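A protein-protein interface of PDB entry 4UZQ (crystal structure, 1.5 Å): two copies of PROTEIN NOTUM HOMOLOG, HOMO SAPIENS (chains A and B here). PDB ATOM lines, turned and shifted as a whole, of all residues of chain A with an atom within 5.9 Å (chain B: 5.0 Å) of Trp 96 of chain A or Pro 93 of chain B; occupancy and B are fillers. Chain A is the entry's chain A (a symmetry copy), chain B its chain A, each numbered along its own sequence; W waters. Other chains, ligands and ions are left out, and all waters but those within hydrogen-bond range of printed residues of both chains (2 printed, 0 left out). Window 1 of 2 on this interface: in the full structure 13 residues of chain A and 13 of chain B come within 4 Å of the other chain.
The indole nitrogen of Trp 96 of chain A lies within hydrogen-bond range of the backbone carbonyl oxygen of Pro 93 of chain B, at 2.9 Å.
The indole nitrogen of Trp 96 of chain B lies within hydrogen-bond range of the backbone carbonyl oxygen of Pro 93 of chain A, 2.9 Å away.
OG of Ser 37 of chain A is in hydrogen-bond range of O of Asn 97 of chain A (2.6 Å).
The backbone NH (N) of Trp 96 of chain B sits close to the side-chain amide nitrogen (ND2) of Asn 92 of chain B, at 3.5 Å.
The side-chain amide nitrogen of Asn 92 of chain A sits close to the backbone NH of Trp 96 of chain A (3.5 Å).
Among the printed residues, merely in contact across the chains: Pro 89 of chain A with Pro 89 of chain B (3.5 Å), Tyr 94 of chain A with Trp 96 of chain B (3.6 Å), Trp 96 of chain A with Tyr 94 of chain B (3.6 Å), Asn 97 of chain A with Tyr 94 of chain B (3.8 Å), Pro 93 of chain A with Pro 89 of chain B (3.8 Å) and Pro 89 of chain A with Pro 93 of chain B (3.8 Å).
Printed residues of chain B within 4 Å of Pro 89 of chain A: Pro 89 and Pro 93.
Trp 96 of chain A touches just these residues of chain B: Pro 93 (2.9 Å) and Tyr 94 (3.6 Å).
Ala 98 of chain A touches none of the printed residues of chain B.
Of chain A, only Pro 89 (3.8 Å) and Trp 96 (2.9 Å) come within 4 Å of Pro 93 of chain B.
Trp 95 of chain B touches none of the printed residues of chain A.
Of the printed residues of chain A, Trp 96 of chain B touches Pro 93 (2.9 Å) and Tyr 94 (3.6 Å).
The nearest printed residue of chain B that does not touch Asn 97 of chain A is Pro 93 of chain B (7.0 Å).
Printed residues of chain B that touch a printed residue of chain A: Pro 89, Pro 93, Tyr 94 and Trp 96.
Hydrophobic or aromatic side chains of chain B within 4 Å of the printed part of chain A: Pro 89, Pro 93, Tyr 94 and Trp 96.
Printed residues of chain A that touch a printed residue of chain B: Pro 89, Pro 93, Tyr 94, Trp 96 and Asn 97.
Hydrophobic or aromatic side chains of chain A that line the printed part of chain B: Pro 89, Pro 93, Tyr 94 and Trp 96.
Pro 89 of chain B touches its own counterpart, Pro 89 of chain A.
Pro 89 of chain A touches Pro 93 of chain B, and with the chains exchanged Pro 93 of chain A touches Pro 89 of chain B.
Pro 93 of chain A touches Trp 96 of chain B, and with the chains exchanged Trp 96 of chain A touches Pro 93 of chain B.
Tyr 94 of chain A touches Trp 96 of chain B, and with the chains exchanged Trp 96 of chain A touches Tyr 94 of chain B.
Positions printed for both chains: 89, 92, 93, 94, 95 and 96.
Water W1 lies within hydrogen-bond range of the side-chain amide oxygen (OD1) of Asn 97 of chain A (2.8 Å) and the side-chain hydroxyl (OH) of Tyr 94 of chain B (3.2 Å).
Water W2 lies within hydrogen-bond range of the backbone carbonyl oxygen (O) of Pro 93 of chain A (2.9 Å), the backbone carbonyl oxygen (O) of Pro 93 of chain B (2.9 Å), the indole nitrogen (NE1) of Trp 96 of chain B (3.5 Å) and the indole nitrogen (NE1) of Trp 96 of chain A (3.5 Å).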
ATOM      1  N   SER A  37     -17.915 -37.747  -7.175  1.00  0.00           N
ATOM      2  CA  SER A  37     -16.551 -37.785  -7.537  1.00  0.00           C
ATOM      3  C   SER A  37     -15.877 -38.960  -6.821  1.00  0.00           C
ATOM      4  O   SER A  37     -15.354 -38.886  -5.667  1.00  0.00           O
ATOM      5  CB  SER A  37     -15.846 -36.509  -7.193  1.00  0.00           C
ATOM      6  OG  SER A  37     -14.541 -36.555  -7.732  1.00  0.00           O
ATOM      7  N   SER A  86     -17.773 -25.764  -8.009  1.00  0.00           N
ATOM      8  CA  SER A  86     -17.344 -26.026  -9.397  1.00  0.00           C
ATOM      9  C   SER A  86     -16.369 -27.186  -9.419  1.00  0.00           C
ATOM     10  O   SER A  86     -15.481 -27.280  -8.551  1.00  0.00           O
ATOM     11  CB  SER A  86     -16.652 -24.804  -9.981  1.00  0.00           C
ATOM     12  OG  SER A  86     -16.169 -25.021 -11.309  1.00  0.00           O
ATOM     13  N   SER A  87     -16.484 -28.001 -10.487  1.00  0.00           N
ATOM     14  CA  SER A  87     -15.522 -29.093 -10.724  1.00  0.00           C
ATOM     15  C   SER A  87     -14.437 -28.630 -11.679  1.00  0.00           C
ATOM     16  O   SER A  87     -13.677 -29.466 -12.122  1.00  0.00           O
ATOM     17  CB  SER A  87     -16.305 -30.272 -11.310  1.00  0.00           C
ATOM     18  OG  SER A  87     -17.229 -30.816 -10.364  1.00  0.00           O
ATOM     19  N   GLN A  88     -14.320 -27.338 -11.965  1.00  0.00           N
ATOM     20  CA  GLN A  88     -13.265 -26.837 -12.822  1.00  0.00           C
ATOM     21  C   GLN A  88     -12.071 -26.351 -12.034  1.00  0.00           C
ATOM     22  O   GLN A  88     -12.182 -25.452 -11.244  1.00  0.00           O
ATOM     23  CB  GLN A  88     -13.783 -25.699 -13.705  1.00  0.00           C
ATOM     24  CG  GLN A  88     -15.060 -26.047 -14.434  1.00  0.00           C
ATOM     25  CD  GLN A  88     -15.008 -27.339 -15.208  1.00  0.00           C
ATOM     26  OE1 GLN A  88     -14.151 -27.525 -16.056  1.00  0.00           O
ATOM     27  NE2 GLN A  88     -15.962 -28.244 -14.936  1.00  0.00           N
ATOM     28  N   PRO A  89     -10.868 -26.935 -12.237  1.00  0.00           N
ATOM     29  CA  PRO A  89      -9.717 -26.522 -11.448  1.00  0.00           C
ATOM     30  C   PRO A  89      -9.434 -25.023 -11.420  1.00  0.00           C
ATOM     31  O   PRO A  89      -9.130 -24.484 -10.349  1.00  0.00           O
ATOM     32  CB  PRO A  89      -8.527 -27.291 -12.138  1.00  0.00           C
ATOM     33  CG  PRO A  89      -9.186 -28.505 -12.640  1.00  0.00           C
ATOM     34  CD  PRO A  89     -10.584 -28.111 -13.067  1.00  0.00           C
ATOM     35  N   ASN A  92     -11.894 -23.535  -8.932  1.00  0.00           N
ATOM     36  CA  ASN A  92     -11.947 -24.078  -7.572  1.00  0.00           C
ATOM     37  C   ASN A  92     -10.594 -24.880  -7.395  1.00  0.00           C
ATOM     38  O   ASN A  92     -10.597 -26.107  -7.447  1.00  0.00           O
ATOM     39  CB  ASN A  92     -13.145 -24.996  -7.484  1.00  0.00           C
ATOM     40  CG  ASN A  92     -13.476 -25.494  -6.066  1.00  0.00           C
ATOM     41  OD1 ASN A  92     -12.869 -25.100  -5.081  1.00  0.00           O
ATOM     42  ND2 ASN A  92     -14.439 -26.429  -6.015  1.00  0.00           N
ATOM     43  N   PRO A  93      -9.525 -24.162  -7.146  1.00  0.00           N
ATOM     44  CA  PRO A  93      -8.224 -24.830  -7.402  1.00  0.00           C
ATOM     45  C   PRO A  93      -7.890 -25.973  -6.487  1.00  0.00           C
ATOM     46  O   PRO A  93      -7.179 -26.913  -6.891  1.00  0.00           O
ATOM     47  CB  PRO A  93      -7.229 -23.678  -7.249  1.00  0.00           C
ATOM     48  CG  PRO A  93      -7.996 -22.423  -7.268  1.00  0.00           C
ATOM     49  CD  PRO A  93      -9.392 -22.692  -6.987  1.00  0.00           C
ATOM     50  N   TYR A  94      -8.303 -25.910  -5.252  1.00  0.00           N
ATOM     51  CA  TYR A  94      -7.941 -26.923  -4.282  1.00  0.00           C
ATOM     52  C   TYR A  94      -8.966 -28.029  -4.234  1.00  0.00           C
ATOM     53  O   TYR A  94      -8.572 -29.202  -4.171  1.00  0.00           O
ATOM     54  CB  TYR A  94      -7.760 -26.392  -2.901  1.00  0.00           C
ATOM     55  CG  TYR A  94      -6.708 -25.359  -2.750  1.00  0.00           C
ATOM     56  CD1 TYR A  94      -6.996 -24.028  -2.998  1.00  0.00           C
ATOM     57  CD2 TYR A  94      -5.363 -25.679  -2.533  1.00  0.00           C
ATOM     58  CE1 TYR A  94      -6.035 -23.030  -2.865  1.00  0.00           C
ATOM     59  CE2 TYR A  94      -4.426 -24.692  -2.378  1.00  0.00           C
ATOM     60  CZ  TYR A  94      -4.736 -23.364  -2.558  1.00  0.00           C
ATOM     61  OH  TYR A  94      -3.778 -22.353  -2.462  1.00  0.00           O
ATOM     62  N   TRP A  95     -10.259 -27.683  -4.340  1.00  0.00           N
ATOM     63  CA  TRP A  95     -11.370 -28.587  -4.055  1.00  0.00           C
ATOM     64  C   TRP A  95     -12.294 -28.966  -5.243  1.00  0.00           C
ATOM     65  O   TRP A  95     -13.373 -29.618  -5.068  1.00  0.00           O
ATOM     66  CB  TRP A  95     -12.196 -28.083  -2.859  1.00  0.00           C
ATOM     67  CG  TRP A  95     -11.391 -27.982  -1.572  1.00  0.00           C
ATOM     68  CD1 TRP A  95     -10.125 -28.514  -1.294  1.00  0.00           C
ATOM     69  CD2 TRP A  95     -11.784 -27.303  -0.392  1.00  0.00           C
ATOM     70  NE1 TRP A  95      -9.763 -28.235   0.006  1.00  0.00           N
ATOM     71  CE2 TRP A  95     -10.752 -27.466   0.574  1.00  0.00           C
ATOM     72  CE3 TRP A  95     -12.909 -26.617  -0.041  1.00  0.00           C
ATOM     73  CZ2 TRP A  95     -10.848 -26.935   1.866  1.00  0.00           C
ATOM     74  CZ3 TRP A  95     -12.990 -26.055   1.229  1.00  0.00           C
ATOM     75  CH2 TRP A  95     -11.972 -26.232   2.163  1.00  0.00           C
ATOM     76  N   TRP A  96     -11.825 -28.675  -6.482  1.00  0.00           N
ATOM     77  CA  TRP A  96     -12.594 -29.013  -7.661  1.00  0.00           C
ATOM     78  C   TRP A  96     -13.049 -30.467  -7.758  1.00  0.00           C
ATOM     79  O   TRP A  96     -14.034 -30.761  -8.385  1.00  0.00           O
ATOM     80  CB  TRP A  96     -11.913 -28.562  -8.957  1.00  0.00           C
ATOM     81  CG  TRP A  96     -10.580 -29.380  -9.164  1.00  0.00           C
ATOM     82  CD1 TRP A  96      -9.365 -29.033  -8.741  1.00  0.00           C
ATOM     83  CD2 TRP A  96     -10.461 -30.662  -9.778  1.00  0.00           C
ATOM     84  NE1 TRP A  96      -8.457 -30.017  -9.089  1.00  0.00           N
ATOM     85  CE2 TRP A  96      -9.120 -31.033  -9.699  1.00  0.00           C
ATOM     86  CE3 TRP A  96     -11.349 -31.496 -10.423  1.00  0.00           C
ATOM     87  CZ2 TRP A  96      -8.652 -32.258 -10.205  1.00  0.00           C
ATOM     88  CZ3 TRP A  96     -10.873 -32.704 -10.951  1.00  0.00           C
ATOM     89  CH2 TRP A  96      -9.556 -33.050 -10.833  1.00  0.00           C
ATOM     90  N   ASN A  97     -12.220 -31.407  -7.231  1.00  0.00           N
ATOM     91  CA  ASN A  97     -12.533 -32.819  -7.353  1.00  0.00           C
ATOM     92  C   ASN A  97     -13.444 -33.404  -6.287  1.00  0.00           C
ATOM     93  O   ASN A  97     -13.681 -34.611  -6.220  1.00  0.00           O
ATOM     94  CB  ASN A  97     -11.226 -33.616  -7.391  1.00  0.00           C
ATOM     95  CG  ASN A  97     -11.386 -34.988  -7.973  1.00  0.00           C
ATOM     96  OD1 ASN A  97     -12.115 -35.203  -8.920  1.00  0.00           O
ATOM     97  ND2 ASN A  97     -10.651 -35.902  -7.452  1.00  0.00           N
ATOM     98  N   ALA A  98     -14.022 -32.546  -5.438  1.00  0.00           N
ATOM     99  CA  ALA A  98     -14.892 -33.062  -4.386  1.00  0.00           C
ATOM    100  C   ALA A  98     -16.222 -33.601  -4.889  1.00  0.00           C
ATOM    101  O   ALA A  98     -16.679 -33.306  -5.992  1.00  0.00           O
ATOM    102  CB  ALA A  98     -15.128 -31.953  -3.378  1.00  0.00           C
ATOM    103  N   MET A 100     -19.892 -33.113  -4.746  1.00  0.00           N
ATOM    104  CA  MET A 100     -20.618 -31.771  -4.646  1.00  0.00           C
ATOM    105  C   MET A 100     -22.094 -32.026  -4.434  1.00  0.00           C
ATOM    106  O   MET A 100     -22.753 -32.753  -5.165  1.00  0.00           O
ATOM    107  CB  MET A 100     -20.492 -30.938  -5.888  1.00  0.00           C
ATOM    108  CG  MET A 100     -19.065 -30.744  -6.349  1.00  0.00           C
ATOM    109  SD  MET A 100     -18.067 -29.865  -5.112  1.00  0.00           S
ATOM    110  CE  MET A 100     -16.586 -29.485  -6.081  1.00  0.00           C
ATOM    111  N   PRO B  89      -3.613 -24.536 -12.147  1.00  0.00           N
ATOM    112  CA  PRO B  89      -4.551 -25.630 -11.943  1.00  0.00           C
ATOM    113  C   PRO B  89      -5.100 -26.280 -13.210  1.00  0.00           C
ATOM    114  O   PRO B  89      -5.186 -27.512 -13.270  1.00  0.00           O
ATOM    115  CB  PRO B  89      -5.714 -24.944 -11.132  1.00  0.00           C
ATOM    116  CG  PRO B  89      -5.003 -23.901 -10.381  1.00  0.00           C
ATOM    117  CD  PRO B  89      -3.886 -23.394 -11.268  1.00  0.00           C
ATOM    118  N   GLU B  90      -5.452 -25.495 -14.227  1.00  0.00           N
ATOM    119  CA  GLU B  90      -5.961 -26.085 -15.457  1.00  0.00           C
ATOM    120  C   GLU B  90      -4.926 -27.022 -16.133  1.00  0.00           C
ATOM    121  O   GLU B  90      -5.322 -28.038 -16.732  1.00  0.00           O
ATOM    122  CB  GLU B  90      -6.408 -25.013 -16.462  1.00  0.00           C
ATOM    123  CG  GLU B  90      -7.348 -25.584 -17.533  1.00  0.00           C
ATOM    124  CD  GLU B  90      -7.947 -24.548 -18.528  1.00  0.00           C
ATOM    125  OE1 GLU B  90      -8.043 -23.330 -18.185  1.00  0.00           O
ATOM    126  OE2 GLU B  90      -8.358 -24.967 -19.659  1.00  0.00           O
ATOM    127  N   GLU B  91      -3.643 -26.682 -16.001  1.00  0.00           N
ATOM    128  CA  GLU B  91      -2.567 -27.496 -16.611  1.00  0.00           C
ATOM    129  C   GLU B  91      -2.209 -28.689 -15.781  1.00  0.00           C
ATOM    130  O   GLU B  91      -1.684 -29.689 -16.323  1.00  0.00           O
ATOM    131  CB  GLU B  91      -1.306 -26.637 -16.805  1.00  0.00           C
ATOM    132  CG  GLU B  91      -0.195 -27.276 -17.667  1.00  0.00           C
ATOM    133  CD  GLU B  91       0.784 -26.241 -18.367  1.00  0.00           C
ATOM    134  OE1 GLU B  91       0.433 -24.962 -18.317  1.00  0.00           O
ATOM    135  OE2 GLU B  91       1.862 -26.637 -19.017  1.00  0.00           O
ATOM    136  N   ASN B  92      -2.374 -28.619 -14.456  1.00  0.00           N
ATOM    137  CA  ASN B  92      -1.834 -29.632 -13.547  1.00  0.00           C
ATOM    138  C   ASN B  92      -2.899 -29.749 -12.382  1.00  0.00           C
ATOM    139  O   ASN B  92      -2.674 -29.235 -11.290  1.00  0.00           O
ATOM    140  CB  ASN B  92      -0.506 -29.130 -13.027  1.00  0.00           C
ATOM    141  CG  ASN B  92       0.303 -30.160 -12.216  1.00  0.00           C
ATOM    142  OD1 ASN B  92      -0.065 -31.317 -12.087  1.00  0.00           O
ATOM    143  ND2 ASN B  92       1.403 -29.663 -11.627  1.00  0.00           N
ATOM    144  N   PRO B  93      -3.972 -30.455 -12.649  1.00  0.00           N
ATOM    145  CA  PRO B  93      -5.138 -30.222 -11.759  1.00  0.00           C
ATOM    146  C   PRO B  93      -4.971 -30.680 -10.338  1.00  0.00           C
ATOM    147  O   PRO B  93      -5.571 -30.095  -9.416  1.00  0.00           O
ATOM    148  CB  PRO B  93      -6.252 -30.991 -12.471  1.00  0.00           C
ATOM    149  CG  PRO B  93      -5.781 -31.302 -13.828  1.00  0.00           C
ATOM    150  CD  PRO B  93      -4.337 -31.183 -13.891  1.00  0.00           C
ATOM    151  N   TYR B  94      -4.246 -31.741 -10.118  1.00  0.00           N
ATOM    152  CA  TYR B  94      -4.115 -32.303  -8.789  1.00  0.00           C
ATOM    153  C   TYR B  94      -2.925 -31.727  -8.064  1.00  0.00           C
ATOM    154  O   TYR B  94      -3.050 -31.415  -6.871  1.00  0.00           O
ATOM    155  CB  TYR B  94      -3.998 -33.788  -8.777  1.00  0.00           C
ATOM    156  CG  TYR B  94      -5.143 -34.521  -9.366  1.00  0.00           C
ATOM    157  CD1 TYR B  94      -5.201 -34.747 -10.731  1.00  0.00           C
ATOM    158  CD2 TYR B  94      -6.284 -34.857  -8.626  1.00  0.00           C
ATOM    159  CE1 TYR B  94      -6.260 -35.433 -11.319  1.00  0.00           C
ATOM    160  CE2 TYR B  94      -7.312 -35.554  -9.205  1.00  0.00           C
ATOM    161  CZ  TYR B  94      -7.329 -35.836 -10.552  1.00  0.00           C
ATOM    162  OH  TYR B  94      -8.398 -36.492 -11.164  1.00  0.00           O
ATOM    163  N   TRP B  95      -1.807 -31.512  -8.776  1.00  0.00           N
ATOM    164  CA  TRP B  95      -0.507 -31.211  -8.181  1.00  0.00           C
ATOM    165  C   TRP B  95       0.097 -29.813  -8.479  1.00  0.00           C
ATOM    166  O   TRP B  95       1.288 -29.515  -8.139  1.00  0.00           O
ATOM    167  CB  TRP B  95       0.509 -32.324  -8.489  1.00  0.00           C
ATOM    168  CG  TRP B  95       0.097 -33.683  -7.942  1.00  0.00           C
ATOM    169  CD1 TRP B  95      -0.910 -33.977  -7.014  1.00  0.00           C
ATOM    170  CD2 TRP B  95       0.668 -34.932  -8.290  1.00  0.00           C
ATOM    171  NE1 TRP B  95      -0.938 -35.330  -6.748  1.00  0.00           N
ATOM    172  CE2 TRP B  95       0.003 -35.944  -7.542  1.00  0.00           C
ATOM    173  CE3 TRP B  95       1.691 -35.292  -9.115  1.00  0.00           C
ATOM    174  CZ2 TRP B  95       0.355 -37.295  -7.637  1.00  0.00           C
ATOM    175  CZ3 TRP B  95       2.018 -36.639  -9.242  1.00  0.00           C
ATOM    176  CH2 TRP B  95       1.360 -37.613  -8.495  1.00  0.00           C
ATOM    177  N   TRP B  96      -0.749 -28.894  -9.006  1.00  0.00           N
ATOM    178  CA  TRP B  96      -0.295 -27.551  -9.294  1.00  0.00           C
ATOM    179  C   TRP B  96       0.387 -26.822  -8.138  1.00  0.00           C
ATOM    180  O   TRP B  96       1.192 -25.953  -8.351  1.00  0.00           O
ATOM    181  CB  TRP B  96      -1.388 -26.682  -9.923  1.00  0.00           C
ATOM    182  CG  TRP B  96      -2.541 -26.442  -8.873  1.00  0.00           C
ATOM    183  CD1 TRP B  96      -3.629 -27.192  -8.708  1.00  0.00           C
ATOM    184  CD2 TRP B  96      -2.578 -25.423  -7.876  1.00  0.00           C
ATOM    185  NE1 TRP B  96      -4.391 -26.679  -7.673  1.00  0.00           N
ATOM    186  CE2 TRP B  96      -3.743 -25.613  -7.136  1.00  0.00           C
ATOM    187  CE3 TRP B  96      -1.764 -24.351  -7.579  1.00  0.00           C
ATOM    188  CZ2 TRP B  96      -4.089 -24.780  -6.058  1.00  0.00           C
ATOM    189  CZ3 TRP B  96      -2.127 -23.506  -6.520  1.00  0.00           C
ATOM    190  CH2 TRP B  96      -3.263 -23.736  -5.797  1.00  0.00           C
ATOM    191  N   THR B 321      -2.427 -33.684 -20.118  1.00  0.00           N
ATOM    192  CA  THR B 321      -3.775 -33.995 -19.643  1.00  0.00           C
ATOM    193  C   THR B 321      -4.674 -34.649 -20.696  1.00  0.00           C
ATOM    194  O   THR B 321      -5.775 -35.166 -20.350  1.00  0.00           O
ATOM    195  CB  THR B 321      -4.475 -32.688 -19.174  1.00  0.00           C
ATOM    196  OG1 THR B 321      -4.337 -31.666 -20.184  1.00  0.00           O
ATOM    197  CG2 THR B 321      -3.830 -32.121 -17.917  1.00  0.00           C
ATOM    198  N   PRO B 331      -2.918 -37.542 -15.251  1.00  0.00           N
ATOM    199  CA  PRO B 331      -2.968 -36.871 -13.945  1.00  0.00           C
ATOM    200  C   PRO B 331      -3.905 -37.613 -12.969  1.00  0.00           C
ATOM    201  O   PRO B 331      -3.579 -37.730 -11.785  1.00  0.00           O
ATOM    202  CB  PRO B 331      -3.389 -35.473 -14.293  1.00  0.00           C
ATOM    203  CG  PRO B 331      -2.924 -35.299 -15.724  1.00  0.00           C
ATOM    204  CD  PRO B 331      -3.164 -36.619 -16.362  1.00  0.00           C
HETATM  205  O   HOH W   1     -11.587 -36.407 -11.363  1.00  0.00           O
HETATM  206  O   HOH W   2      -6.051 -29.539  -6.644  1.00  0.00           O
